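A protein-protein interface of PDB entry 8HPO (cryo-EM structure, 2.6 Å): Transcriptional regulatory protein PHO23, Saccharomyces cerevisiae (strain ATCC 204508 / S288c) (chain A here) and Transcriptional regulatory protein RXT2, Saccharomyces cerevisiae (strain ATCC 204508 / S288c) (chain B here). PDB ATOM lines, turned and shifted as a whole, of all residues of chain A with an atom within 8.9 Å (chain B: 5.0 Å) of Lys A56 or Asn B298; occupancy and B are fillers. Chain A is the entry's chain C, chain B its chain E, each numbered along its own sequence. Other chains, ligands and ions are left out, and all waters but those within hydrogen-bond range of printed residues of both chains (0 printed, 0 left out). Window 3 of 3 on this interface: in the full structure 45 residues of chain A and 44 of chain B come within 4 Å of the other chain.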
ATOM      1  N   ARG A  49      -0.161 -15.206  17.309  1.00  0.00           N
ATOM      2  CA  ARG A  49      -1.109 -16.249  16.939  1.00  0.00           C
ATOM      3  C   ARG A  49      -2.322 -16.267  17.859  1.00  0.00           C
ATOM      4  O   ARG A  49      -3.425 -16.600  17.418  1.00  0.00           O
ATOM      5  CB  ARG A  49      -0.419 -17.611  16.945  1.00  0.00           C
ATOM      6  CG  ARG A  49       0.787 -17.690  16.028  1.00  0.00           C
ATOM      7  CD  ARG A  49       0.530 -18.572  14.832  1.00  0.00           C
ATOM      8  NE  ARG A  49       1.687 -18.631  13.946  1.00  0.00           N
ATOM      9  CZ  ARG A  49       2.541 -19.648  13.896  1.00  0.00           C
ATOM     10  NH1 ARG A  49       2.370 -20.696  14.684  1.00  0.00           N
ATOM     11  NH2 ARG A  49       3.568 -19.618  13.061  1.00  0.00           N
ATOM     12  N   ILE A  50      -2.156 -15.890  19.126  1.00  0.00           N
ATOM     13  CA  ILE A  50      -3.303 -15.882  20.025  1.00  0.00           C
ATOM     14  C   ILE A  50      -4.263 -14.769  19.646  1.00  0.00           C
ATOM     15  O   ILE A  50      -5.478 -14.979  19.583  1.00  0.00           O
ATOM     16  CB  ILE A  50      -2.852 -15.765  21.489  1.00  0.00           C
ATOM     17  CG1 ILE A  50      -2.365 -17.117  21.994  1.00  0.00           C
ATOM     18  CG2 ILE A  50      -3.991 -15.269  22.349  1.00  0.00           C
ATOM     19  CD1 ILE A  50      -2.102 -17.150  23.480  1.00  0.00           C
ATOM     20  N   ASP A  51      -3.744 -13.577  19.353  1.00  0.00           N
ATOM     21  CA  ASP A  51      -4.652 -12.501  18.967  1.00  0.00           C
ATOM     22  C   ASP A  51      -5.264 -12.764  17.596  1.00  0.00           C
ATOM     23  O   ASP A  51      -6.411 -12.373  17.336  1.00  0.00           O
ATOM     24  CB  ASP A  51      -3.929 -11.159  18.998  1.00  0.00           C
ATOM     25  CG  ASP A  51      -4.339 -10.316  20.183  1.00  0.00           C
ATOM     26  OD1 ASP A  51      -5.446 -10.548  20.709  1.00  0.00           O
ATOM     27  OD2 ASP A  51      -3.559  -9.431  20.589  1.00  0.00           O
ATOM     28  N   LYS A  52      -4.538 -13.465  16.724  1.00  0.00           N
ATOM     29  CA  LYS A  52      -5.100 -13.831  15.427  1.00  0.00           C
ATOM     30  C   LYS A  52      -6.249 -14.814  15.586  1.00  0.00           C
ATOM     31  O   LYS A  52      -7.346 -14.584  15.069  1.00  0.00           O
ATOM     32  CB  LYS A  52      -4.014 -14.417  14.527  1.00  0.00           C
ATOM     33  CG  LYS A  52      -4.399 -14.498  13.061  1.00  0.00           C
ATOM     34  CD  LYS A  52      -3.276 -15.106  12.236  1.00  0.00           C
ATOM     35  CE  LYS A  52      -3.699 -15.346  10.797  1.00  0.00           C
ATOM     36  NZ  LYS A  52      -3.668 -14.104   9.975  1.00  0.00           N
ATOM     37  N   PHE A  53      -6.017 -15.914  16.308  1.00  0.00           N
ATOM     38  CA  PHE A  53      -7.079 -16.880  16.565  1.00  0.00           C
ATOM     39  C   PHE A  53      -8.251 -16.234  17.291  1.00  0.00           C
ATOM     40  O   PHE A  53      -9.404 -16.623  17.085  1.00  0.00           O
ATOM     41  CB  PHE A  53      -6.527 -18.057  17.367  1.00  0.00           C
ATOM     42  CG  PHE A  53      -7.575 -19.025  17.837  1.00  0.00           C
ATOM     43  CD1 PHE A  53      -8.221 -18.840  19.048  1.00  0.00           C
ATOM     44  CD2 PHE A  53      -7.903 -20.128  17.075  1.00  0.00           C
ATOM     45  CE1 PHE A  53      -9.177 -19.725  19.477  1.00  0.00           C
ATOM     46  CE2 PHE A  53      -8.856 -21.015  17.501  1.00  0.00           C
ATOM     47  CZ  PHE A  53      -9.495 -20.815  18.705  1.00  0.00           C
ATOM     48  N   LEU A  54      -7.981 -15.248  18.146  1.00  0.00           N
ATOM     49  CA  LEU A  54      -9.066 -14.562  18.825  1.00  0.00           C
ATOM     50  C   LEU A  54      -9.867 -13.681  17.884  1.00  0.00           C
ATOM     51  O   LEU A  54     -11.070 -13.510  18.097  1.00  0.00           O
ATOM     52  CB  LEU A  54      -8.529 -13.721  19.980  1.00  0.00           C
ATOM     53  CG  LEU A  54      -8.497 -14.414  21.339  1.00  0.00           C
ATOM     54  CD1 LEU A  54      -8.651 -13.403  22.456  1.00  0.00           C
ATOM     55  CD2 LEU A  54      -9.575 -15.465  21.418  1.00  0.00           C
ATOM     56  N   LYS A  55      -9.239 -13.127  16.850  1.00  0.00           N
ATOM     57  CA  LYS A  55      -9.976 -12.253  15.943  1.00  0.00           C
ATOM     58  C   LYS A  55      -9.984 -12.778  14.514  1.00  0.00           C
ATOM     59  O   LYS A  55      -9.752 -12.020  13.569  1.00  0.00           O
ATOM     60  CB  LYS A  55      -9.404 -10.838  15.991  1.00  0.00           C
ATOM     61  CG  LYS A  55      -9.683 -10.128  17.302  1.00  0.00           C
ATOM     62  CD  LYS A  55     -11.109 -10.385  17.760  1.00  0.00           C
ATOM     63  CE  LYS A  55     -11.290 -10.047  19.228  1.00  0.00           C
ATOM     64  NZ  LYS A  55     -12.700 -10.231  19.672  1.00  0.00           N
ATOM     65  N   LYS A  56     -10.245 -14.071  14.351  1.00  0.00           N
ATOM     66  CA  LYS A  56     -10.443 -14.659  13.029  1.00  0.00           C
ATOM     67  C   LYS A  56     -11.903 -14.547  12.598  1.00  0.00           C
ATOM     68  O   LYS A  56     -12.201 -14.228  11.447  1.00  0.00           O
ATOM     69  CB  LYS A  56     -10.007 -16.124  13.018  1.00  0.00           C
ATOM     70  CG  LYS A  56     -10.195 -16.809  11.676  1.00  0.00           C
ATOM     71  CD  LYS A  56      -9.356 -16.153  10.593  1.00  0.00           C
ATOM     72  CE  LYS A  56     -10.125 -16.052   9.283  1.00  0.00           C
ATOM     73  NZ  LYS A  56     -10.447 -17.389   8.710  1.00  0.00           N
ATOM     74  N   GLN A  63     -10.952 -24.657   8.560  1.00  0.00           N
ATOM     75  CA  GLN A  63     -10.111 -25.626   7.866  1.00  0.00           C
ATOM     76  C   GLN A  63      -8.635 -25.395   8.182  1.00  0.00           C
ATOM     77  O   GLN A  63      -7.852 -26.339   8.273  1.00  0.00           O
ATOM     78  CB  GLN A  63     -10.349 -25.564   6.352  1.00  0.00           C
ATOM     79  CG  GLN A  63     -10.224 -24.177   5.733  1.00  0.00           C
ATOM     80  CD  GLN A  63     -11.509 -23.382   5.824  1.00  0.00           C
ATOM     81  OE1 GLN A  63     -12.504 -23.716   5.180  1.00  0.00           O
ATOM     82  NE2 GLN A  63     -11.497 -22.323   6.625  1.00  0.00           N
ATOM     83  N   THR A  64      -8.260 -24.126   8.333  1.00  0.00           N
ATOM     84  CA  THR A  64      -6.916 -23.769   8.765  1.00  0.00           C
ATOM     85  C   THR A  64      -6.840 -23.474  10.254  1.00  0.00           C
ATOM     86  O   THR A  64      -5.760 -23.601  10.847  1.00  0.00           O
ATOM     87  CB  THR A  64      -6.412 -22.553   7.984  1.00  0.00           C
ATOM     88  OG1 THR A  64      -6.776 -21.353   8.678  1.00  0.00           O
ATOM     89  CG2 THR A  64      -7.022 -22.529   6.595  1.00  0.00           C
ATOM     90  N   GLN A  65      -7.960 -23.087  10.867  1.00  0.00           N
ATOM     91  CA  GLN A  65      -7.964 -22.789  12.294  1.00  0.00           C
ATOM     92  C   GLN A  65      -7.567 -24.006  13.120  1.00  0.00           C
ATOM     93  O   GLN A  65      -7.058 -23.862  14.237  1.00  0.00           O
ATOM     94  CB  GLN A  65      -9.340 -22.276  12.711  1.00  0.00           C
ATOM     95  CG  GLN A  65      -9.318 -21.391  13.936  1.00  0.00           C
ATOM     96  CD  GLN A  65      -9.243 -19.925  13.581  1.00  0.00           C
ATOM     97  OE1 GLN A  65      -8.893 -19.569  12.458  1.00  0.00           O
ATOM     98  NE2 GLN A  65      -9.573 -19.064  14.535  1.00  0.00           N
ATOM     99  N   VAL A  66      -7.769 -25.211  12.584  1.00  0.00           N
ATOM    100  CA  VAL A  66      -7.279 -26.400  13.273  1.00  0.00           C
ATOM    101  C   VAL A  66      -5.757 -26.389  13.338  1.00  0.00           C
ATOM    102  O   VAL A  66      -5.164 -26.622  14.400  1.00  0.00           O
ATOM    103  CB  VAL A  66      -7.819 -27.668  12.589  1.00  0.00           C
ATOM    104  CG1 VAL A  66      -7.703 -27.551  11.084  1.00  0.00           C
ATOM    105  CG2 VAL A  66      -7.084 -28.899  13.087  1.00  0.00           C
ATOM    106  N   LEU A  68      -3.928 -23.759  13.145  1.00  0.00           N
ATOM    107  CA  LEU A  68      -3.551 -22.647  14.010  1.00  0.00           C
ATOM    108  C   LEU A  68      -3.599 -23.048  15.479  1.00  0.00           C
ATOM    109  O   LEU A  68      -2.656 -22.778  16.232  1.00  0.00           O
ATOM    110  CB  LEU A  68      -4.459 -21.450  13.751  1.00  0.00           C
ATOM    111  CG  LEU A  68      -3.851 -20.069  13.988  1.00  0.00           C
ATOM    112  CD1 LEU A  68      -4.551 -19.027  13.132  1.00  0.00           C
ATOM    113  CD2 LEU A  68      -3.921 -19.694  15.455  1.00  0.00           C
ATOM    114  N   GLU B 224     -15.584 -11.574  24.123  1.00  0.00           N
ATOM    115  CA  GLU B 224     -15.969 -10.501  23.230  1.00  0.00           C
ATOM    116  C   GLU B 224     -16.955  -9.570  23.930  1.00  0.00           C
ATOM    117  O   GLU B 224     -17.638  -9.968  24.874  1.00  0.00           O
ATOM    118  CB  GLU B 224     -16.608 -11.064  21.962  1.00  0.00           C
ATOM    119  CG  GLU B 224     -15.630 -11.501  20.898  1.00  0.00           C
ATOM    120  CD  GLU B 224     -15.448 -13.003  20.865  1.00  0.00           C
ATOM    121  OE1 GLU B 224     -15.798 -13.663  21.867  1.00  0.00           O
ATOM    122  OE2 GLU B 224     -14.963 -13.523  19.838  1.00  0.00           O
ATOM    123  N   GLN B 296     -22.474 -17.949  19.859  1.00  0.00           N
ATOM    124  CA  GLN B 296     -21.230 -18.679  20.078  1.00  0.00           C
ATOM    125  C   GLN B 296     -20.063 -17.728  19.871  1.00  0.00           C
ATOM    126  O   GLN B 296     -20.192 -16.747  19.133  1.00  0.00           O
ATOM    127  CB  GLN B 296     -21.111 -19.877  19.133  1.00  0.00           C
ATOM    128  CG  GLN B 296     -20.201 -20.983  19.629  1.00  0.00           C
ATOM    129  CD  GLN B 296     -20.931 -22.012  20.470  1.00  0.00           C
ATOM    130  OE1 GLN B 296     -22.023 -21.755  20.980  1.00  0.00           O
ATOM    131  NE2 GLN B 296     -20.332 -23.187  20.619  1.00  0.00           N
ATOM    132  N   SER B 297     -18.923 -18.002  20.498  1.00  0.00           N
ATOM    133  CA  SER B 297     -17.726 -17.231  20.198  1.00  0.00           C
ATOM    134  C   SER B 297     -17.330 -17.466  18.747  1.00  0.00           C
ATOM    135  O   SER B 297     -17.354 -18.601  18.265  1.00  0.00           O
ATOM    136  CB  SER B 297     -16.590 -17.622  21.138  1.00  0.00           C
ATOM    137  OG  SER B 297     -16.645 -16.867  22.334  1.00  0.00           O
ATOM    138  N   ASN B 298     -16.986 -16.388  18.041  1.00  0.00           N
ATOM    139  CA  ASN B 298     -16.627 -16.532  16.636  1.00  0.00           C
ATOM    140  C   ASN B 298     -15.360 -17.355  16.465  1.00  0.00           C
ATOM    141  O   ASN B 298     -15.224 -18.083  15.475  1.00  0.00           O
ATOM    142  CB  ASN B 298     -16.460 -15.163  15.984  1.00  0.00           C
ATOM    143  CG  ASN B 298     -16.582 -15.220  14.477  1.00  0.00           C
ATOM    144  OD1 ASN B 298     -15.587 -15.359  13.768  1.00  0.00           O
ATOM    145  ND2 ASN B 298     -17.808 -15.115  13.980  1.00  0.00           N
ATOM    146  N   ALA B 299     -14.439 -17.268  17.425  1.00  0.00           N
ATOM    147  CA  ALA B 299     -13.238 -18.094  17.378  1.00  0.00           C
ATOM    148  C   ALA B 299     -13.589 -19.575  17.415  1.00  0.00           C
ATOM    149  O   ALA B 299     -12.933 -20.392  16.758  1.00  0.00           O
ATOM    150  CB  ALA B 299     -12.311 -17.732  18.534  1.00  0.00           C
ATOM    151  N   LEU B 300     -14.625 -19.938  18.171  1.00  0.00           N
ATOM    152  CA  LEU B 300     -14.992 -21.343  18.308  1.00  0.00           C
ATOM    153  C   LEU B 300     -15.854 -21.826  17.149  1.00  0.00           C
ATOM    154  O   LEU B 300     -15.727 -22.980  16.727  1.00  0.00           O
ATOM    155  CB  LEU B 300     -15.726 -21.568  19.628  1.00  0.00           C
ATOM    156  CG  LEU B 300     -14.889 -21.804  20.881  1.00  0.00           C
ATOM    157  CD1 LEU B 300     -15.812 -21.988  22.064  1.00  0.00           C
ATOM    158  CD2 LEU B 300     -13.977 -23.006  20.711  1.00  0.00           C
ATOM    159  N   LEU B 301     -16.745 -20.973  16.635  1.00  0.00           N
ATOM    160  CA  LEU B 301     -17.599 -21.401  15.532  1.00  0.00           C
ATOM    161  C   LEU B 301     -16.878 -21.292  14.199  1.00  0.00           C
ATOM    162  O   LEU B 301     -17.380 -21.785  13.184  1.00  0.00           O
ATOM    163  CB  LEU B 301     -18.900 -20.595  15.502  1.00  0.00           C
ATOM    164  CG  LEU B 301     -18.859 -19.088  15.238  1.00  0.00           C
ATOM    165  CD1 LEU B 301     -19.238 -18.791  13.801  1.00  0.00           C
ATOM    166  CD2 LEU B 301     -19.796 -18.354  16.179  1.00  0.00           C
ATOM    167  N   SER B 302     -15.708 -20.651  14.174  1.00  0.00           N
ATOM    168  CA  SER B 302     -14.927 -20.603  12.946  1.00  0.00           C
ATOM    169  C   SER B 302     -14.163 -21.896  12.707  1.00  0.00           C
ATOM    170  O   SER B 302     -13.697 -22.129  11.587  1.00  0.00           O
ATOM    171  CB  SER B 302     -13.960 -19.423  12.982  1.00  0.00           C
ATOM    172  OG  SER B 302     -13.512 -19.187  14.305  1.00  0.00           O
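O of Phe A53 touches CB of Ala B299, 3.4 Å away. Lys A56 touches Asn B298 (C to OD1, 3.9 Å). Gln A65 touches Ser B302 (NE2 to OG, 3.9 Å).
Printed residues of chain A that touch a printed residue of chain B: Phe A53, Lys A55, Lys A56 and Gln A65. Hydrophobic or aromatic side chains of chain A that line the printed part of chain B: Phe A53. Of the 8 printed residues of chain B, 4 touch a printed residue of chain A. Printed residues of chain B that touch a printed residue of chain A: Glu B224, Asn B298, Ala B299 and Ser B302. Among the printed residues, Asp or Glu carboxylates within 4 Å of a Lys or Arg side-chain nitrogen of the other chain: Lys A55 with Glu B224.
Of the printed residues of chain B, Phe A53 touches Ala B299. Printed residues of chain B within 4 Å of Lys A55: Glu B224 (3.4 Å). Lys A56 touches just one residue of chain B: Asn B298. Of the printed residues of chain B, Gln A65 touches Ser B302. Leu A68 touches none of the printed residues of chain B. Of the printed residues of chain A, Glu B224 touches Lys A55. No residue of chain A comes within 4 Å of Ser B297. Asn B298 touches just one residue of chain A: Lys A56. Printed residues of chain A within 4 Å of Ala B299: Phe A53 (3.4 Å). Leu B300 touches none of the printed residues of chain A. Of the printed residues of chain A, Ser B302 touches Gln A65 (3.9 Å). The nearest residue of chain B that does not touch Lys A56 is Ser B302 (4.8 Å).
The side-chain carboxylate of Glu B224 lies within salt-bridge range of the side-chain amino group of Lys A55 (3.998 Å).
The backbone carbonyl oxygen of Ala B299 lies within hydrogen-bond range of the side-chain hydroxyl of Ser B302. OE1 of Glu B224 lies within hydrogen-bond range of OG of Ser B297, 3.3 Å away.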
